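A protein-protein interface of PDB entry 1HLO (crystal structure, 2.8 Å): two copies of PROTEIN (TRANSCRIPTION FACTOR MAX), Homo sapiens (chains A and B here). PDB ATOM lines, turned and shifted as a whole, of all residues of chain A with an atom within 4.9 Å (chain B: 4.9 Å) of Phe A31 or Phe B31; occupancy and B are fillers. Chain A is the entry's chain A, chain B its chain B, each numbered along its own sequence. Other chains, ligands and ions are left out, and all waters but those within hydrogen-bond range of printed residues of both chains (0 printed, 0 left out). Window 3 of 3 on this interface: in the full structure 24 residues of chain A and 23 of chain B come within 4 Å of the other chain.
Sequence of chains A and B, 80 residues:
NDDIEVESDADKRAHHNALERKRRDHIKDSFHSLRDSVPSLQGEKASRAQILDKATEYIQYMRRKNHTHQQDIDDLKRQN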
ATOM      1  N   ILE A  27      17.210 -36.261 -10.545  1.00  0.00           N
ATOM      2  CA  ILE A  27      17.452 -34.908 -10.990  1.00  0.00           C
ATOM      3  C   ILE A  27      16.660 -33.881 -10.202  1.00  0.00           C
ATOM      4  O   ILE A  27      17.171 -32.819  -9.847  1.00  0.00           O
ATOM      5  CB  ILE A  27      17.186 -34.802 -12.466  1.00  0.00           C
ATOM      6  CG1 ILE A  27      18.199 -35.661 -13.189  1.00  0.00           C
ATOM      7  CG2 ILE A  27      17.255 -33.354 -12.940  1.00  0.00           C
ATOM      8  CD1 ILE A  27      17.957 -35.691 -14.630  1.00  0.00           C
ATOM      9  N   LYS A  28      15.409 -34.193  -9.908  1.00  0.00           N
ATOM     10  CA  LYS A  28      14.584 -33.261  -9.161  1.00  0.00           C
ATOM     11  C   LYS A  28      15.252 -33.051  -7.820  1.00  0.00           C
ATOM     12  O   LYS A  28      15.304 -31.955  -7.278  1.00  0.00           O
ATOM     13  CB  LYS A  28      13.199 -33.831  -8.991  1.00  0.00           C
ATOM     14  CG  LYS A  28      12.286 -33.018  -8.133  1.00  0.00           C
ATOM     15  CD  LYS A  28      10.939 -33.711  -8.127  1.00  0.00           C
ATOM     16  CE  LYS A  28       9.870 -32.947  -7.370  1.00  0.00           C
ATOM     17  NZ  LYS A  28       8.505 -33.530  -7.655  1.00  0.00           N
ATOM     18  N   ASP A  29      15.865 -34.099  -7.324  1.00  0.00           N
ATOM     19  CA  ASP A  29      16.518 -33.959  -6.059  1.00  0.00           C
ATOM     20  C   ASP A  29      17.729 -33.095  -6.193  1.00  0.00           C
ATOM     21  O   ASP A  29      17.866 -32.140  -5.447  1.00  0.00           O
ATOM     22  CB  ASP A  29      16.858 -35.312  -5.489  1.00  0.00           C
ATOM     23  CG  ASP A  29      15.948 -35.678  -4.356  1.00  0.00           C
ATOM     24  OD1 ASP A  29      16.310 -36.601  -3.602  1.00  0.00           O
ATOM     25  OD2 ASP A  29      14.875 -35.030  -4.203  1.00  0.00           O
ATOM     26  N   SER A  30      18.570 -33.391  -7.181  1.00  0.00           N
ATOM     27  CA  SER A  30      19.763 -32.614  -7.427  1.00  0.00           C
ATOM     28  C   SER A  30      19.492 -31.133  -7.677  1.00  0.00           C
ATOM     29  O   SER A  30      20.282 -30.291  -7.318  1.00  0.00           O
ATOM     30  CB  SER A  30      20.514 -33.249  -8.558  1.00  0.00           C
ATOM     31  OG  SER A  30      20.916 -34.544  -8.128  1.00  0.00           O
ATOM     32  N   PHE A  31      18.360 -30.804  -8.269  1.00  0.00           N
ATOM     33  CA  PHE A  31      18.014 -29.405  -8.476  1.00  0.00           C
ATOM     34  C   PHE A  31      17.724 -28.807  -7.091  1.00  0.00           C
ATOM     35  O   PHE A  31      17.999 -27.642  -6.837  1.00  0.00           O
ATOM     36  CB  PHE A  31      16.738 -29.289  -9.334  1.00  0.00           C
ATOM     37  CG  PHE A  31      16.993 -28.993 -10.785  1.00  0.00           C
ATOM     38  CD1 PHE A  31      17.480 -27.758 -11.180  1.00  0.00           C
ATOM     39  CD2 PHE A  31      16.774 -29.971 -11.754  1.00  0.00           C
ATOM     40  CE1 PHE A  31      17.739 -27.497 -12.532  1.00  0.00           C
ATOM     41  CE2 PHE A  31      17.033 -29.713 -13.114  1.00  0.00           C
ATOM     42  CZ  PHE A  31      17.521 -28.471 -13.497  1.00  0.00           C
ATOM     43  N   HIS A  32      17.127 -29.601  -6.209  1.00  0.00           N
ATOM     44  CA  HIS A  32      16.778 -29.136  -4.876  1.00  0.00           C
ATOM     45  C   HIS A  32      18.029 -28.717  -4.132  1.00  0.00           C
ATOM     46  O   HIS A  32      18.131 -27.581  -3.637  1.00  0.00           O
ATOM     47  CB  HIS A  32      16.074 -30.249  -4.112  1.00  0.00           C
ATOM     48  CG  HIS A  32      15.459 -29.808  -2.815  1.00  0.00           C
ATOM     49  ND1 HIS A  32      14.129 -30.015  -2.521  1.00  0.00           N
ATOM     50  CD2 HIS A  32      15.992 -29.172  -1.740  1.00  0.00           C
ATOM     51  CE1 HIS A  32      13.862 -29.520  -1.321  1.00  0.00           C
ATOM     52  NE2 HIS A  32      14.974 -29.004  -0.828  1.00  0.00           N
ATOM     53  N   SER A  33      18.965 -29.651  -4.019  1.00  0.00           N
ATOM     54  CA  SER A  33      20.221 -29.391  -3.354  1.00  0.00           C
ATOM     55  C   SER A  33      21.004 -28.222  -3.957  1.00  0.00           C
ATOM     56  O   SER A  33      21.652 -27.503  -3.213  1.00  0.00           O
ATOM     57  CB  SER A  33      21.057 -30.633  -3.379  1.00  0.00           C
ATOM     58  OG  SER A  33      20.340 -31.709  -2.803  1.00  0.00           O
ATOM     59  N   LEU A  34      20.993 -28.044  -5.285  1.00  0.00           N
ATOM     60  CA  LEU A  34      21.690 -26.893  -5.898  1.00  0.00           C
ATOM     61  C   LEU A  34      20.958 -25.634  -5.416  1.00  0.00           C
ATOM     62  O   LEU A  34      21.572 -24.689  -4.962  1.00  0.00           O
ATOM     63  CB  LEU A  34      21.610 -26.909  -7.424  1.00  0.00           C
ATOM     64  CG  LEU A  34      22.823 -26.461  -8.242  1.00  0.00           C
ATOM     65  CD1 LEU A  34      22.426 -26.108  -9.707  1.00  0.00           C
ATOM     66  CD2 LEU A  34      23.511 -25.356  -7.558  1.00  0.00           C
ATOM     67  N   ARG A  35      19.637 -25.659  -5.466  1.00  0.00           N
ATOM     68  CA  ARG A  35      18.835 -24.538  -5.046  1.00  0.00           C
ATOM     69  C   ARG A  35      19.264 -24.082  -3.667  1.00  0.00           C
ATOM     70  O   ARG A  35      19.596 -22.920  -3.478  1.00  0.00           O
ATOM     71  CB  ARG A  35      17.339 -24.919  -5.010  1.00  0.00           C
ATOM     72  CG  ARG A  35      16.469 -23.686  -5.080  1.00  0.00           C
ATOM     73  CD  ARG A  35      15.095 -23.885  -4.575  1.00  0.00           C
ATOM     74  NE  ARG A  35      15.118 -24.210  -3.162  1.00  0.00           N
ATOM     75  CZ  ARG A  35      14.573 -25.311  -2.663  1.00  0.00           C
ATOM     76  NH1 ARG A  35      13.984 -26.176  -3.474  1.00  0.00           N
ATOM     77  NH2 ARG A  35      14.578 -25.525  -1.354  1.00  0.00           N
ATOM     78  N   ARG A  48      13.660 -24.427 -12.837  1.00  0.00           N
ATOM     79  CA  ARG A  48      14.904 -25.072 -13.176  1.00  0.00           C
ATOM     80  C   ARG A  48      15.842 -24.152 -13.940  1.00  0.00           C
ATOM     81  O   ARG A  48      17.038 -24.167 -13.690  1.00  0.00           O
ATOM     82  CB  ARG A  48      14.640 -26.357 -13.960  1.00  0.00           C
ATOM     83  CG  ARG A  48      14.212 -27.563 -13.104  1.00  0.00           C
ATOM     84  CD  ARG A  48      13.396 -28.538 -13.960  1.00  0.00           C
ATOM     85  NE  ARG A  48      13.838 -29.940 -14.001  1.00  0.00           N
ATOM     86  CZ  ARG A  48      13.514 -30.855 -13.087  1.00  0.00           C
ATOM     87  NH1 ARG A  48      12.740 -30.521 -12.051  1.00  0.00           N
ATOM     88  NH2 ARG A  48      13.996 -32.096 -13.192  1.00  0.00           N
ATOM     89  N   ILE A  51      17.559 -21.727 -11.404  1.00  0.00           N
ATOM     90  CA  ILE A  51      18.515 -22.422 -10.570  1.00  0.00           C
ATOM     91  C   ILE A  51      19.830 -22.560 -11.336  1.00  0.00           C
ATOM     92  O   ILE A  51      20.868 -22.199 -10.828  1.00  0.00           O
ATOM     93  CB  ILE A  51      17.994 -23.808 -10.187  1.00  0.00           C
ATOM     94  CG1 ILE A  51      16.683 -23.675  -9.389  1.00  0.00           C
ATOM     95  CG2 ILE A  51      19.055 -24.566  -9.438  1.00  0.00           C
ATOM     96  CD1 ILE A  51      16.276 -24.905  -8.677  1.00  0.00           C
ATOM     97  N   LEU A  52      19.789 -23.039 -12.573  1.00  0.00           N
ATOM     98  CA  LEU A  52      20.988 -23.201 -13.386  1.00  0.00           C
ATOM     99  C   LEU A  52      21.638 -21.865 -13.625  1.00  0.00           C
ATOM    100  O   LEU A  52      22.849 -21.726 -13.477  1.00  0.00           O
ATOM    101  CB  LEU A  52      20.645 -23.795 -14.737  1.00  0.00           C
ATOM    102  CG  LEU A  52      20.640 -25.292 -15.036  1.00  0.00           C
ATOM    103  CD1 LEU A  52      21.161 -26.062 -13.874  1.00  0.00           C
ATOM    104  CD2 LEU A  52      19.270 -25.737 -15.383  1.00  0.00           C
ATOM    105  N   ILE B  27      17.069 -24.558 -20.945  1.00  0.00           N
ATOM    106  CA  ILE B  27      17.686 -25.413 -19.941  1.00  0.00           C
ATOM    107  C   ILE B  27      18.931 -26.123 -20.466  1.00  0.00           C
ATOM    108  O   ILE B  27      19.892 -26.337 -19.737  1.00  0.00           O
ATOM    109  CB  ILE B  27      16.661 -26.426 -19.424  1.00  0.00           C
ATOM    110  CG1 ILE B  27      15.550 -25.671 -18.723  1.00  0.00           C
ATOM    111  CG2 ILE B  27      17.283 -27.421 -18.460  1.00  0.00           C
ATOM    112  CD1 ILE B  27      14.447 -26.533 -18.251  1.00  0.00           C
ATOM    113  N   LYS B  28      18.924 -26.482 -21.739  1.00  0.00           N
ATOM    114  CA  LYS B  28      20.063 -27.166 -22.353  1.00  0.00           C
ATOM    115  C   LYS B  28      21.253 -26.208 -22.369  1.00  0.00           C
ATOM    116  O   LYS B  28      22.354 -26.565 -21.966  1.00  0.00           O
ATOM    117  CB  LYS B  28      19.681 -27.569 -23.771  1.00  0.00           C
ATOM    118  CG  LYS B  28      20.622 -28.491 -24.514  1.00  0.00           C
ATOM    119  CD  LYS B  28      20.110 -28.723 -25.970  1.00  0.00           C
ATOM    120  CE  LYS B  28      18.591 -29.131 -26.014  1.00  0.00           C
ATOM    121  NZ  LYS B  28      17.946 -29.201 -27.386  1.00  0.00           N
ATOM    122  N   ASP B  29      21.017 -24.967 -22.770  1.00  0.00           N
ATOM    123  CA  ASP B  29      22.084 -24.014 -22.829  1.00  0.00           C
ATOM    124  C   ASP B  29      22.604 -23.714 -21.469  1.00  0.00           C
ATOM    125  O   ASP B  29      23.816 -23.768 -21.220  1.00  0.00           O
ATOM    126  CB  ASP B  29      21.640 -22.769 -23.542  1.00  0.00           C
ATOM    127  CG  ASP B  29      22.200 -22.695 -24.926  1.00  0.00           C
ATOM    128  OD1 ASP B  29      22.205 -21.574 -25.464  1.00  0.00           O
ATOM    129  OD2 ASP B  29      22.663 -23.736 -25.472  1.00  0.00           O
ATOM    130  N   SER B  30      21.681 -23.483 -20.555  1.00  0.00           N
ATOM    131  CA  SER B  30      22.042 -23.195 -19.169  1.00  0.00           C
ATOM    132  C   SER B  30      22.851 -24.299 -18.509  1.00  0.00           C
ATOM    133  O   SER B  30      23.698 -24.001 -17.683  1.00  0.00           O
ATOM    134  CB  SER B  30      20.799 -22.835 -18.369  1.00  0.00           C
ATOM    135  OG  SER B  30      20.276 -21.618 -18.898  1.00  0.00           O
ATOM    136  N   PHE B  31      22.633 -25.555 -18.903  1.00  0.00           N
ATOM    137  CA  PHE B  31      23.400 -26.672 -18.359  1.00  0.00           C
ATOM    138  C   PHE B  31      24.832 -26.543 -18.909  1.00  0.00           C
ATOM    139  O   PHE B  31      25.816 -26.824 -18.223  1.00  0.00           O
ATOM    140  CB  PHE B  31      22.810 -28.001 -18.824  1.00  0.00           C
ATOM    141  CG  PHE B  31      21.924 -28.681 -17.813  1.00  0.00           C
ATOM    142  CD1 PHE B  31      22.462 -29.244 -16.653  1.00  0.00           C
ATOM    143  CD2 PHE B  31      20.551 -28.755 -18.016  1.00  0.00           C
ATOM    144  CE1 PHE B  31      21.634 -29.875 -15.709  1.00  0.00           C
ATOM    145  CE2 PHE B  31      19.729 -29.378 -17.072  1.00  0.00           C
ATOM    146  CZ  PHE B  31      20.272 -29.937 -15.922  1.00  0.00           C
ATOM    147  N   HIS B  32      24.948 -26.051 -20.137  1.00  0.00           N
ATOM    148  CA  HIS B  32      26.243 -25.896 -20.775  1.00  0.00           C
ATOM    149  C   HIS B  32      27.081 -24.943 -19.983  1.00  0.00           C
ATOM    150  O   HIS B  32      28.146 -25.287 -19.505  1.00  0.00           O
ATOM    151  CB  HIS B  32      26.086 -25.379 -22.197  1.00  0.00           C
ATOM    152  CG  HIS B  32      27.337 -25.474 -23.013  1.00  0.00           C
ATOM    153  ND1 HIS B  32      27.408 -26.187 -24.188  1.00  0.00           N
ATOM    154  CD2 HIS B  32      28.570 -24.950 -22.819  1.00  0.00           C
ATOM    155  CE1 HIS B  32      28.631 -26.103 -24.685  1.00  0.00           C
ATOM    156  NE2 HIS B  32      29.356 -25.357 -23.872  1.00  0.00           N
ATOM    157  N   SER B  33      26.573 -23.745 -19.827  1.00  0.00           N
ATOM    158  CA  SER B  33      27.262 -22.727 -19.089  1.00  0.00           C
ATOM    159  C   SER B  33      27.606 -23.140 -17.674  1.00  0.00           C
ATOM    160  O   SER B  33      28.668 -22.775 -17.180  1.00  0.00           O
ATOM    161  CB  SER B  33      26.423 -21.462 -19.077  1.00  0.00           C
ATOM    162  OG  SER B  33      26.142 -21.062 -20.402  1.00  0.00           O
ATOM    163  N   LEU B  34      26.715 -23.851 -16.989  1.00  0.00           N
ATOM    164  CA  LEU B  34      27.029 -24.270 -15.618  1.00  0.00           C
ATOM    165  C   LEU B  34      28.210 -25.215 -15.754  1.00  0.00           C
ATOM    166  O   LEU B  34      29.182 -25.091 -15.032  1.00  0.00           O
ATOM    167  CB  LEU B  34      25.880 -25.041 -14.958  1.00  0.00           C
ATOM    168  CG  LEU B  34      25.590 -24.835 -13.469  1.00  0.00           C
ATOM    169  CD1 LEU B  34      24.800 -26.009 -12.892  1.00  0.00           C
ATOM    170  CD2 LEU B  34      26.834 -24.629 -12.706  1.00  0.00           C
ATOM    171  N   ARG B  35      28.153 -26.089 -16.753  1.00  0.00           N
ATOM    172  CA  ARG B  35      29.193 -27.081 -16.952  1.00  0.00           C
ATOM    173  C   ARG B  35      30.550 -26.437 -17.021  1.00  0.00           C
ATOM    174  O   ARG B  35      31.476 -26.802 -16.309  1.00  0.00           O
ATOM    175  CB  ARG B  35      28.953 -27.881 -18.242  1.00  0.00           C
ATOM    176  CG  ARG B  35      29.618 -29.240 -18.183  1.00  0.00           C
ATOM    177  CD  ARG B  35      29.908 -29.865 -19.523  1.00  0.00           C
ATOM    178  NE  ARG B  35      30.785 -29.026 -20.315  1.00  0.00           N
ATOM    179  CZ  ARG B  35      30.415 -28.507 -21.473  1.00  0.00           C
ATOM    180  NH1 ARG B  35      29.200 -28.760 -21.931  1.00  0.00           N
ATOM    181  NH2 ARG B  35      31.243 -27.758 -22.182  1.00  0.00           N
ATOM    182  N   ARG B  48      23.410 -34.824 -17.032  1.00  0.00           N
ATOM    183  CA  ARG B  48      22.796 -33.686 -16.385  1.00  0.00           C
ATOM    184  C   ARG B  48      22.854 -33.893 -14.864  1.00  0.00           C
ATOM    185  O   ARG B  48      23.050 -32.936 -14.123  1.00  0.00           O
ATOM    186  CB  ARG B  48      21.348 -33.513 -16.869  1.00  0.00           C
ATOM    187  CG  ARG B  48      21.202 -32.806 -18.213  1.00  0.00           C
ATOM    188  CD  ARG B  48      19.897 -33.205 -18.854  1.00  0.00           C
ATOM    189  NE  ARG B  48      18.981 -32.110 -19.200  1.00  0.00           N
ATOM    190  CZ  ARG B  48      19.019 -31.423 -20.345  1.00  0.00           C
ATOM    191  NH1 ARG B  48      19.949 -31.702 -21.262  1.00  0.00           N
ATOM    192  NH2 ARG B  48      18.089 -30.491 -20.599  1.00  0.00           N
ATOM    193  N   ILE B  51      26.420 -32.895 -13.646  1.00  0.00           N
ATOM    194  CA  ILE B  51      26.606 -31.458 -13.701  1.00  0.00           C
ATOM    195  C   ILE B  51      25.986 -30.849 -12.461  1.00  0.00           C
ATOM    196  O   ILE B  51      26.632 -30.080 -11.768  1.00  0.00           O
ATOM    197  CB  ILE B  51      25.927 -30.856 -14.958  1.00  0.00           C
ATOM    198  CG1 ILE B  51      26.535 -31.448 -16.232  1.00  0.00           C
ATOM    199  CG2 ILE B  51      26.008 -29.345 -14.945  1.00  0.00           C
ATOM    200  CD1 ILE B  51      26.241 -30.663 -17.453  1.00  0.00           C
ATOM    201  N   LEU B  52      24.741 -31.211 -12.160  1.00  0.00           N
ATOM    202  CA  LEU B  52      24.046 -30.662 -10.999  1.00  0.00           C
ATOM    203  C   LEU B  52      24.776 -31.022  -9.725  1.00  0.00           C
ATOM    204  O   LEU B  52      24.970 -30.199  -8.861  1.00  0.00           O
ATOM    205  CB  LEU B  52      22.638 -31.224 -10.929  1.00  0.00           C
ATOM    206  CG  LEU B  52      21.431 -30.520 -11.536  1.00  0.00           C
ATOM    207  CD1 LEU B  52      21.728 -29.155 -12.090  1.00  0.00           C
ATOM    208  CD2 LEU B  52      20.856 -31.421 -12.562  1.00  0.00           C
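Of the printed residues of chain B, Ser A30 touches Leu B52.
Printed residues of chain B within 4 Å of Phe A31: Phe B31.
Arg A48 touches none of the printed residues of chain B.
Of the printed residues of chain B, Leu A52 touches Ser B30 (3.8 Å), Leu B34 (3.8 Å) and Leu B52 (3.6 Å).
Phe B31 touches one residue of chain A.
Of the printed residues of chain A, Leu B34 touches Leu A34 (3.97 Å) and Leu A52 (3.8 Å).
The nearest residue of chain B that does not touch Phe A31 is Leu B52 (4.2 Å).
Among the printed residues, merely in contact across the chains: Leu A52 with Leu B52 (3.6 Å), Leu A52 with Ser B30 (3.8 Å), Leu A52 with Leu B34 (3.8 Å), Ser A30 with Leu B52 (3.8 Å), Leu A34 with Leu B52 (3.9 Å), Phe A31 with Phe B31 (3.9 Å) and Leu A34 with Leu B34 (3.97 Å).
Phe A31 touches its own counterpart, Phe B31.
Leu A34 touches its own counterpart, Leu B34.
Leu A34 touches Leu B52, and with the chains exchanged Leu A52 touches Leu B34.
Leu B52 touches its own counterpart, Leu A52.
Positions printed for both chains: 27, 28, 29, 30, 31, 32, 33, 34, 35, 48, 51 and 52.
Of the 7 pairs that touch across the chains among the printed residues, 7 have their exchanged pair printed and touching as well.
Of the 12 printed residues of chain A, 4 touch a printed residue of chain B.
Along chain B the printed residues that touch a printed residue of chain A span positions 30 to 52.
Among the printed residues, 7 pairs touch across the chains.
Among the printed residues, no Asp or Glu carboxylate lies within 4 Å of a Lys or Arg side-chain nitrogen of the other chain.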
